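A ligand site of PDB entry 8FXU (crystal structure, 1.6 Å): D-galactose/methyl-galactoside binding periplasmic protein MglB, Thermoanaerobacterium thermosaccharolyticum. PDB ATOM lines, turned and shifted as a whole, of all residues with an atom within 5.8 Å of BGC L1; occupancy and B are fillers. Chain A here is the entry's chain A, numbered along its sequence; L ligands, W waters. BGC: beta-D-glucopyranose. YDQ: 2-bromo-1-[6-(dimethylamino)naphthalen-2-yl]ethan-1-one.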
ATOM      1  N   TYR A  11       0.176 -10.632  18.336  1.00  0.00           N
ATOM      2  CA  TYR A  11      -0.215 -11.533  19.442  1.00  0.00           C
ATOM      3  C   TYR A  11       0.641 -12.806  19.431  1.00  0.00           C
ATOM      4  O   TYR A  11       1.030 -13.288  20.487  1.00  0.00           O
ATOM      5  CB  TYR A  11      -1.736 -11.833  19.421  1.00  0.00           C
ATOM      6  CG  TYR A  11      -2.143 -13.090  18.672  1.00  0.00           C
ATOM      7  CD1 TYR A  11      -2.328 -13.085  17.290  1.00  0.00           C
ATOM      8  CD2 TYR A  11      -2.358 -14.291  19.353  1.00  0.00           C
ATOM      9  CE1 TYR A  11      -2.702 -14.249  16.598  1.00  0.00           C
ATOM     10  CE2 TYR A  11      -2.730 -15.456  18.675  1.00  0.00           C
ATOM     11  CZ  TYR A  11      -2.885 -15.429  17.300  1.00  0.00           C
ATOM     12  OH  TYR A  11      -3.251 -16.586  16.657  1.00  0.00           O
ATOM     13  N   ASP A  15       1.399 -17.178  13.515  1.00  0.00           N
ATOM     14  CA  ASP A  15       0.022 -17.108  13.038  1.00  0.00           C
ATOM     15  C   ASP A  15       0.109 -16.724  11.560  1.00  0.00           C
ATOM     16  O   ASP A  15       0.724 -15.706  11.223  1.00  0.00           O
ATOM     17  CB  ASP A  15      -0.782 -16.090  13.846  1.00  0.00           C
ATOM     18  CG  ASP A  15      -2.241 -15.969  13.384  1.00  0.00           C
ATOM     19  OD1 ASP A  15      -2.515 -15.241  12.399  1.00  0.00           O
ATOM     20  OD2 ASP A  15      -3.112 -16.572  14.031  1.00  0.00           O
ATOM     21  N   CYS A  17      -2.151 -15.666   9.185  1.00  0.00           N
ATOM     22  CA  CYS A  17      -2.717 -14.371   8.837  1.00  0.00           C
ATOM     23  C   CYS A  17      -1.922 -13.186   9.392  1.00  0.00           C
ATOM     24  O   CYS A  17      -1.619 -12.236   8.660  1.00  0.00           O
ATOM     25  CB  CYS A  17      -4.167 -14.305   9.327  1.00  0.00           C
ATOM     26  SG  CYS A  17      -4.925 -12.654   9.418  1.00  0.00           S
ATOM     27  N   MET A  18      -1.547 -13.238  10.669  1.00  0.00           N
ATOM     28  CA  MET A  18      -0.900 -12.064  11.253  1.00  0.00           C
ATOM     29  C   MET A  18       0.517 -11.896  10.713  1.00  0.00           C
ATOM     30  O   MET A  18       1.084 -10.808  10.789  1.00  0.00           O
ATOM     31  CB  MET A  18      -0.919 -12.131  12.772  1.00  0.00           C
ATOM     32  CG  MET A  18      -2.302 -11.846  13.364  1.00  0.00           C
ATOM     33  SD  MET A  18      -3.060 -10.324  12.733  1.00  0.00           S
ATOM     34  CE  MET A  18      -1.825  -9.139  13.196  1.00  0.00           C
ATOM     35  N   ASN A  65      -1.862  -5.619  18.711  1.00  0.00           N
ATOM     36  CA  ASN A  65      -2.718  -6.753  18.376  1.00  0.00           C
ATOM     37  C   ASN A  65      -2.869  -7.554  19.687  1.00  0.00           C
ATOM     38  O   ASN A  65      -2.030  -8.392  20.004  1.00  0.00           O
ATOM     39  CB  ASN A  65      -2.032  -7.528  17.228  1.00  0.00           C
ATOM     40  CG  ASN A  65      -2.736  -8.815  16.803  1.00  0.00           C
ATOM     41  OD1 ASN A  65      -2.076  -9.859  16.695  1.00  0.00           O
ATOM     42  ND2 ASN A  65      -4.020  -8.755  16.501  1.00  0.00           N
ATOM     43  N   ASN A  90      -7.125  -6.159  14.636  1.00  0.00           N
ATOM     44  CA  ASN A  90      -7.408  -7.594  14.384  1.00  0.00           C
ATOM     45  C   ASN A  90      -8.054  -8.358  15.547  1.00  0.00           C
ATOM     46  O   ASN A  90      -8.891  -9.229  15.324  1.00  0.00           O
ATOM     47  CB  ASN A  90      -6.138  -8.317  13.914  1.00  0.00           C
ATOM     48  CG  ASN A  90      -6.296  -9.842  13.946  1.00  0.00           C
ATOM     49  OD1 ASN A  90      -5.885 -10.498  14.910  1.00  0.00           O
ATOM     50  ND2 ASN A  90      -6.905 -10.416  12.907  1.00  0.00           N
ATOM     51  N   ARG A  91      -7.670  -8.040  16.790  1.00  0.00           N
ATOM     52  CA  ARG A  91      -8.314  -8.589  17.976  1.00  0.00           C
ATOM     53  C   ARG A  91      -8.971  -7.406  18.678  1.00  0.00           C
ATOM     54  O   ARG A  91      -8.285  -6.475  19.096  1.00  0.00           O
ATOM     55  CB  ARG A  91      -7.298  -9.341  18.848  1.00  0.00           C
ATOM     56  CG  ARG A  91      -6.725 -10.551  18.096  1.00  0.00           C
ATOM     57  CD  ARG A  91      -5.351 -11.008  18.588  1.00  0.00           C
ATOM     58  NE  ARG A  91      -5.418 -11.923  19.734  1.00  0.00           N
ATOM     59  CZ  ARG A  91      -5.614 -13.230  19.665  1.00  0.00           C
ATOM     60  NH1 ARG A  91      -5.796 -13.834  18.482  1.00  0.00           N
ATOM     61  NH2 ARG A  91      -5.637 -13.947  20.778  1.00  0.00           N
ATOM     62  N   GLN A 148     -10.066 -19.097  18.774  1.00  0.00           N
ATOM     63  CA  GLN A 148      -9.867 -19.039  20.211  1.00  0.00           C
ATOM     64  C   GLN A 148     -11.143 -18.608  20.929  1.00  0.00           C
ATOM     65  O   GLN A 148     -11.852 -17.716  20.467  1.00  0.00           O
ATOM     66  CB  GLN A 148      -8.734 -18.065  20.562  1.00  0.00           C
ATOM     67  CG  GLN A 148      -7.356 -18.564  20.134  1.00  0.00           C
ATOM     68  CD  GLN A 148      -6.312 -17.462  20.194  1.00  0.00           C
ATOM     69  OE1 GLN A 148      -6.497 -16.370  19.638  1.00  0.00           O
ATOM     70  NE2 GLN A 148      -5.197 -17.731  20.900  1.00  0.00           N
ATOM     71  N   HIS A 151     -12.618 -14.754  21.187  1.00  0.00           N
ATOM     72  CA  HIS A 151     -12.169 -13.896  20.092  1.00  0.00           C
ATOM     73  C   HIS A 151     -13.404 -13.487  19.293  1.00  0.00           C
ATOM     74  O   HIS A 151     -14.222 -14.345  18.969  1.00  0.00           O
ATOM     75  CB  HIS A 151     -11.162 -14.707  19.270  1.00  0.00           C
ATOM     76  CG  HIS A 151     -10.446 -13.949  18.199  1.00  0.00           C
ATOM     77  ND1 HIS A 151     -11.083 -13.298  17.153  1.00  0.00           N
ATOM     78  CD2 HIS A 151      -9.115 -13.800  17.974  1.00  0.00           C
ATOM     79  CE1 HIS A 151     -10.180 -12.796  16.334  1.00  0.00           C
ATOM     80  NE2 HIS A 151      -8.980 -13.083  16.813  1.00  0.00           N
ATOM     81  N   ASP A 153     -13.929 -12.794  16.221  1.00  0.00           N
ATOM     82  CA  ASP A 153     -14.092 -13.440  14.938  1.00  0.00           C
ATOM     83  C   ASP A 153     -14.577 -14.882  15.108  1.00  0.00           C
ATOM     84  O   ASP A 153     -15.330 -15.373  14.280  1.00  0.00           O
ATOM     85  CB  ASP A 153     -12.780 -13.442  14.156  1.00  0.00           C
ATOM     86  CG  ASP A 153     -12.365 -12.042  13.710  1.00  0.00           C
ATOM     87  OD1 ASP A 153     -13.190 -11.110  13.745  1.00  0.00           O
ATOM     88  OD2 ASP A 153     -11.191 -11.876  13.318  1.00  0.00           O
ATOM     89  N   ARG A 157     -18.084 -15.489  13.436  1.00  0.00           N
ATOM     90  CA  ARG A 157     -18.060 -16.359  12.259  1.00  0.00           C
ATOM     91  C   ARG A 157     -18.830 -17.639  12.528  1.00  0.00           C
ATOM     92  O   ARG A 157     -19.532 -18.133  11.644  1.00  0.00           O
ATOM     93  CB  ARG A 157     -16.630 -16.673  11.837  1.00  0.00           C
ATOM     94  CG  ARG A 157     -15.934 -15.496  11.179  1.00  0.00           C
ATOM     95  CD  ARG A 157     -14.470 -15.799  10.990  1.00  0.00           C
ATOM     96  NE  ARG A 157     -13.722 -14.622  10.548  1.00  0.00           N
ATOM     97  CZ  ARG A 157     -12.391 -14.543  10.573  1.00  0.00           C
ATOM     98  NH1 ARG A 157     -11.676 -15.560  11.006  1.00  0.00           N
ATOM     99  NH2 ARG A 157     -11.779 -13.439  10.166  1.00  0.00           N
ATOM    100  N   TRP A 182      -7.285 -21.384  16.057  1.00  0.00           N
ATOM    101  CA  TRP A 182      -6.728 -20.860  14.793  1.00  0.00           C
ATOM    102  C   TRP A 182      -5.582 -21.714  14.272  1.00  0.00           C
ATOM    103  O   TRP A 182      -4.958 -21.365  13.260  1.00  0.00           O
ATOM    104  CB  TRP A 182      -6.212 -19.409  14.935  1.00  0.00           C
ATOM    105  CG  TRP A 182      -7.169 -18.438  15.561  1.00  0.00           C
ATOM    106  CD1 TRP A 182      -6.985 -17.718  16.706  1.00  0.00           C
ATOM    107  CD2 TRP A 182      -8.451 -18.037  15.046  1.00  0.00           C
ATOM    108  NE1 TRP A 182      -8.074 -16.929  16.955  1.00  0.00           N
ATOM    109  CE2 TRP A 182      -8.994 -17.091  15.953  1.00  0.00           C
ATOM    110  CE3 TRP A 182      -9.190 -18.389  13.916  1.00  0.00           C
ATOM    111  CZ2 TRP A 182     -10.232 -16.491  15.754  1.00  0.00           C
ATOM    112  CZ3 TRP A 182     -10.437 -17.805  13.717  1.00  0.00           C
ATOM    113  CH2 TRP A 182     -10.943 -16.855  14.642  1.00  0.00           C
ATOM    114  N   ASN A 208     -13.388 -21.560  11.264  1.00  0.00           N
ATOM    115  CA  ASN A 208     -13.367 -20.106  11.390  1.00  0.00           C
ATOM    116  C   ASN A 208     -12.176 -19.474  10.639  1.00  0.00           C
ATOM    117  O   ASN A 208     -12.165 -18.266  10.425  1.00  0.00           O
ATOM    118  CB  ASN A 208     -13.291 -19.644  12.855  1.00  0.00           C
ATOM    119  CG  ASN A 208     -14.556 -19.906  13.697  1.00  0.00           C
ATOM    120  OD1 ASN A 208     -14.464 -19.723  14.895  1.00  0.00           O
ATOM    121  ND2 ASN A 208     -15.685 -20.293  13.101  1.00  0.00           N
ATOM    122  N   ASN A 209     -11.140 -20.259  10.296  1.00  0.00           N
ATOM    123  CA  ASN A 209     -10.091 -19.711   9.423  1.00  0.00           C
ATOM    124  C   ASN A 209      -9.491 -20.789   8.524  1.00  0.00           C
ATOM    125  O   ASN A 209      -9.809 -21.978   8.646  1.00  0.00           O
ATOM    126  CB  ASN A 209      -8.975 -18.990  10.235  1.00  0.00           C
ATOM    127  CG  ASN A 209      -7.974 -19.956  10.900  1.00  0.00           C
ATOM    128  OD1 ASN A 209      -8.224 -21.160  11.012  1.00  0.00           O
ATOM    129  ND2 ASN A 209      -6.849 -19.398  11.372  1.00  0.00           N
ATOM    130  N   ASP A 210      -8.637 -20.348   7.611  1.00  0.00           N
ATOM    131  CA  ASP A 210      -8.044 -21.241   6.633  1.00  0.00           C
ATOM    132  C   ASP A 210      -7.111 -22.253   7.264  1.00  0.00           C
ATOM    133  O   ASP A 210      -7.114 -23.408   6.875  1.00  0.00           O
ATOM    134  CB  ASP A 210      -7.300 -20.460   5.554  1.00  0.00           C
ATOM    135  CG  ASP A 210      -8.239 -19.878   4.498  1.00  0.00           C
ATOM    136  OD1 ASP A 210      -9.474 -20.076   4.585  1.00  0.00           O
ATOM    137  OD2 ASP A 210      -7.723 -19.205   3.583  1.00  0.00           O
ATOM    138  N   VAL A 237     -11.875 -19.118   6.236  1.00  0.00           N
ATOM    139  CA  VAL A 237     -11.797 -17.656   6.114  1.00  0.00           C
ATOM    140  C   VAL A 237     -10.312 -17.276   6.090  1.00  0.00           C
ATOM    141  O   VAL A 237      -9.554 -17.791   6.930  1.00  0.00           O
ATOM    142  CB  VAL A 237     -12.470 -16.890   7.280  1.00  0.00           C
ATOM    143  CG1 VAL A 237     -12.176 -15.412   7.142  1.00  0.00           C
ATOM    144  CG2 VAL A 237     -13.971 -17.122   7.293  1.00  0.00           C
ATOM    145  N   ASP A 238      -9.933 -16.414   5.132  1.00  0.00           N
ATOM    146  CA  ASP A 238      -8.706 -15.593   5.106  1.00  0.00           C
ATOM    147  C   ASP A 238      -8.210 -15.440   3.672  1.00  0.00           C
ATOM    148  O   ASP A 238      -7.783 -14.369   3.268  1.00  0.00           O
ATOM    149  CB  ASP A 238      -7.547 -16.161   5.946  1.00  0.00           C
ATOM    150  CG  ASP A 238      -7.701 -15.897   7.437  1.00  0.00           C
ATOM    151  OD1 ASP A 238      -8.503 -15.035   7.848  1.00  0.00           O
ATOM    152  OD2 ASP A 238      -7.024 -16.610   8.215  1.00  0.00           O
ATOM    153  N   ASN A 258      -9.631 -12.071   3.743  1.00  0.00           N
ATOM    154  CA  ASN A 258      -9.417 -11.170   4.861  1.00  0.00           C
ATOM    155  C   ASN A 258      -8.306 -10.273   4.377  1.00  0.00           C
ATOM    156  O   ASN A 258      -7.173 -10.723   4.174  1.00  0.00           O
ATOM    157  CB  ASN A 258      -9.044 -11.944   6.132  1.00  0.00           C
ATOM    158  CG  ASN A 258      -9.099 -11.078   7.390  1.00  0.00           C
ATOM    159  OD1 ASN A 258      -9.620  -9.947   7.377  1.00  0.00           O
ATOM    160  ND2 ASN A 258      -8.597 -11.619   8.493  1.00  0.00           N
ATOM    161  N   TYR A 299     -14.697  -7.728   3.716  1.00  0.00           N
ATOM    162  CA  TYR A 299     -14.413  -9.105   3.335  1.00  0.00           C
ATOM    163  C   TYR A 299     -14.919  -9.361   1.933  1.00  0.00           C
ATOM    164  O   TYR A 299     -15.841  -8.691   1.485  1.00  0.00           O
ATOM    165  CB  TYR A 299     -15.111 -10.054   4.276  1.00  0.00           C
ATOM    166  CG  TYR A 299     -14.475 -10.238   5.624  1.00  0.00           C
ATOM    167  CD1 TYR A 299     -13.315 -10.991   5.757  1.00  0.00           C
ATOM    168  CD2 TYR A 299     -15.066  -9.721   6.776  1.00  0.00           C
ATOM    169  CE1 TYR A 299     -12.742 -11.207   7.001  1.00  0.00           C
ATOM    170  CE2 TYR A 299     -14.508  -9.935   8.036  1.00  0.00           C
ATOM    171  CZ  TYR A 299     -13.329 -10.685   8.132  1.00  0.00           C
ATOM    172  OH  TYR A 299     -12.737 -10.912   9.358  1.00  0.00           O
HETATM  173  C2  BGC L   1      -7.941 -14.644  11.220  1.00  0.00           C
HETATM  174  C3  BGC L   1      -7.218 -15.842  11.790  1.00  0.00           C
HETATM  175  C4  BGC L   1      -6.194 -15.378  12.814  1.00  0.00           C
HETATM  176  C5  BGC L   1      -6.824 -14.478  13.861  1.00  0.00           C
HETATM  177  C6  BGC L   1      -5.760 -13.955  14.823  1.00  0.00           C
HETATM  178  C1  BGC L   1      -8.514 -13.811  12.361  1.00  0.00           C
HETATM  179  O1  BGC L   1      -9.158 -12.670  11.812  1.00  0.00           O
HETATM  180  O2  BGC L   1      -8.991 -15.077  10.352  1.00  0.00           O
HETATM  181  O3  BGC L   1      -6.533 -16.559  10.763  1.00  0.00           O
HETATM  182  O4  BGC L   1      -5.633 -16.530  13.429  1.00  0.00           O
HETATM  183  O5  BGC L   1      -7.460 -13.387  13.227  1.00  0.00           O
HETATM  184  O6  BGC L   1      -6.271 -12.916  15.650  1.00  0.00           O
HETATM  185  C10 YDQ L   2      -3.032 -13.092   5.368  1.00  0.00           C
HETATM  186  C13 YDQ L   2      -4.532 -13.507   3.028  1.00  0.00           C
HETATM  187  C01 YDQ L   2       1.045 -14.338   0.380  1.00  0.00           C
HETATM  188  C03 YDQ L   2      -1.216 -14.514  -0.733  1.00  0.00           C
HETATM  189  C04 YDQ L   2      -1.060 -13.963   1.713  1.00  0.00           C
HETATM  190  C05 YDQ L   2      -2.447 -13.879   1.762  1.00  0.00           C
HETATM  191  C06 YDQ L   2      -3.106 -13.589   2.997  1.00  0.00           C
HETATM  192  C07 YDQ L   2      -2.369 -13.392   4.132  1.00  0.00           C
HETATM  193  C08 YDQ L   2      -0.945 -13.472   4.086  1.00  0.00           C
HETATM  194  C09 YDQ L   2      -0.311 -13.755   2.876  1.00  0.00           C
HETATM  195  C11 YDQ L   2      -4.419 -13.015   5.388  1.00  0.00           C
HETATM  196  C12 YDQ L   2      -5.168 -13.223   4.225  1.00  0.00           C
HETATM  197  C14 YDQ L   2      -5.148 -12.730   6.687  1.00  0.00           C
HETATM  198  C16 YDQ L   2      -4.482 -11.936   7.794  1.00  0.00           C
HETATM  199  N02 YDQ L   2      -0.414 -14.265   0.450  1.00  0.00           N
HETATM  200  O15 YDQ L   2      -6.236 -13.166   6.868  1.00  0.00           O
HETATM  201  O   HOH W   1      -3.990 -17.598  10.519  1.00  0.00           O
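NH1 of Arg 91 is in hydrogen-bond range of O6 of BGC L1 (3.0 Å). C16 of YDQ L2 is covalently linked to SG of Cys 17 (1.8 Å). The side-chain carboxylate (OD2) of Asp 15 is in hydrogen-bond range of an oxygen (O4) of BGC L1, at 2.6 Å. The side-chain carboxylate (OD2) of Asp 153 is in hydrogen-bond range of an oxygen (O1) of BGC L1, 2.7 Å away. The side-chain amide nitrogen of Asn 258 sits close to an oxygen (O15) of YDQ L2 (3.3 Å). A ring nitrogen (NE2) of His 151 sits at hydrogen-bond distance from an oxygen (O6) of BGC L1. An oxygen (O3) of BGC L1 lies within hydrogen-bond range of the side-chain amide nitrogen of Asn 209 (2.9 Å). The guanidinium group of Arg 157 lies within hydrogen-bond range of an oxygen (O2) of BGC L1, 2.8 Å away. An oxygen (O6) of BGC L1 is in hydrogen-bond range of the side-chain amide oxygen (OD1) of Asn 90, 2.6 Å away. The side-chain carboxylate (OD1) of Asp 238 is in hydrogen-bond range of an oxygen (O2) of BGC L1, at 2.6 Å.
Water W1 lies within hydrogen-bond range of an oxygen (O3) of BGC L1, the backbone NH of Cys 17, the side-chain carboxylate of Asp 15 and the side-chain amide nitrogen of Asn 209.
NH1 of Arg 157 is in hydrogen-bond range of O of Asn 208 (2.8 Å). The side-chain hydroxyl (OH) of Tyr 299 sits at hydrogen-bond distance from the guanidinium group (NH2) of Arg 157, 2.8 Å away. OD1 of Asp 15 is in hydrogen-bond range of N of Met 18 (2.8 Å). The side-chain amide nitrogen (ND2) of Asn 65 sits at hydrogen-bond distance from the side-chain amide oxygen (OD1) of Asn 90 (3.0 Å). The side-chain amide oxygen of Asn 90 lies close to the side-chain sulfur of Met 18 (3.6 Å). NH2 of Arg 91 is in hydrogen-bond range of OE1 of Gln 148 (2.8 Å). NH2 of Arg 157 lies within salt-bridge range of OD2 of Asp 153 (3.6 Å). NE1 of Trp 182 lies within hydrogen-bond range of OE1 of Gln 148 (3.2 Å).
Residues that only touch BGC L1: Tyr 11, Cys 17, Trp 182 and Asn 258. Hydrophobic or aromatic side chains within 4 Å of BGC L1: Tyr 11, His 151 and Trp 182. 12 residues have an atom within 4 Å of BGC L1: Tyr 11, Asp 15, Cys 17, Asn 90, Arg 91, His 151, Asp 153, Arg 157, Trp 182, Asn 209, Asp 238 and Asn 258.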
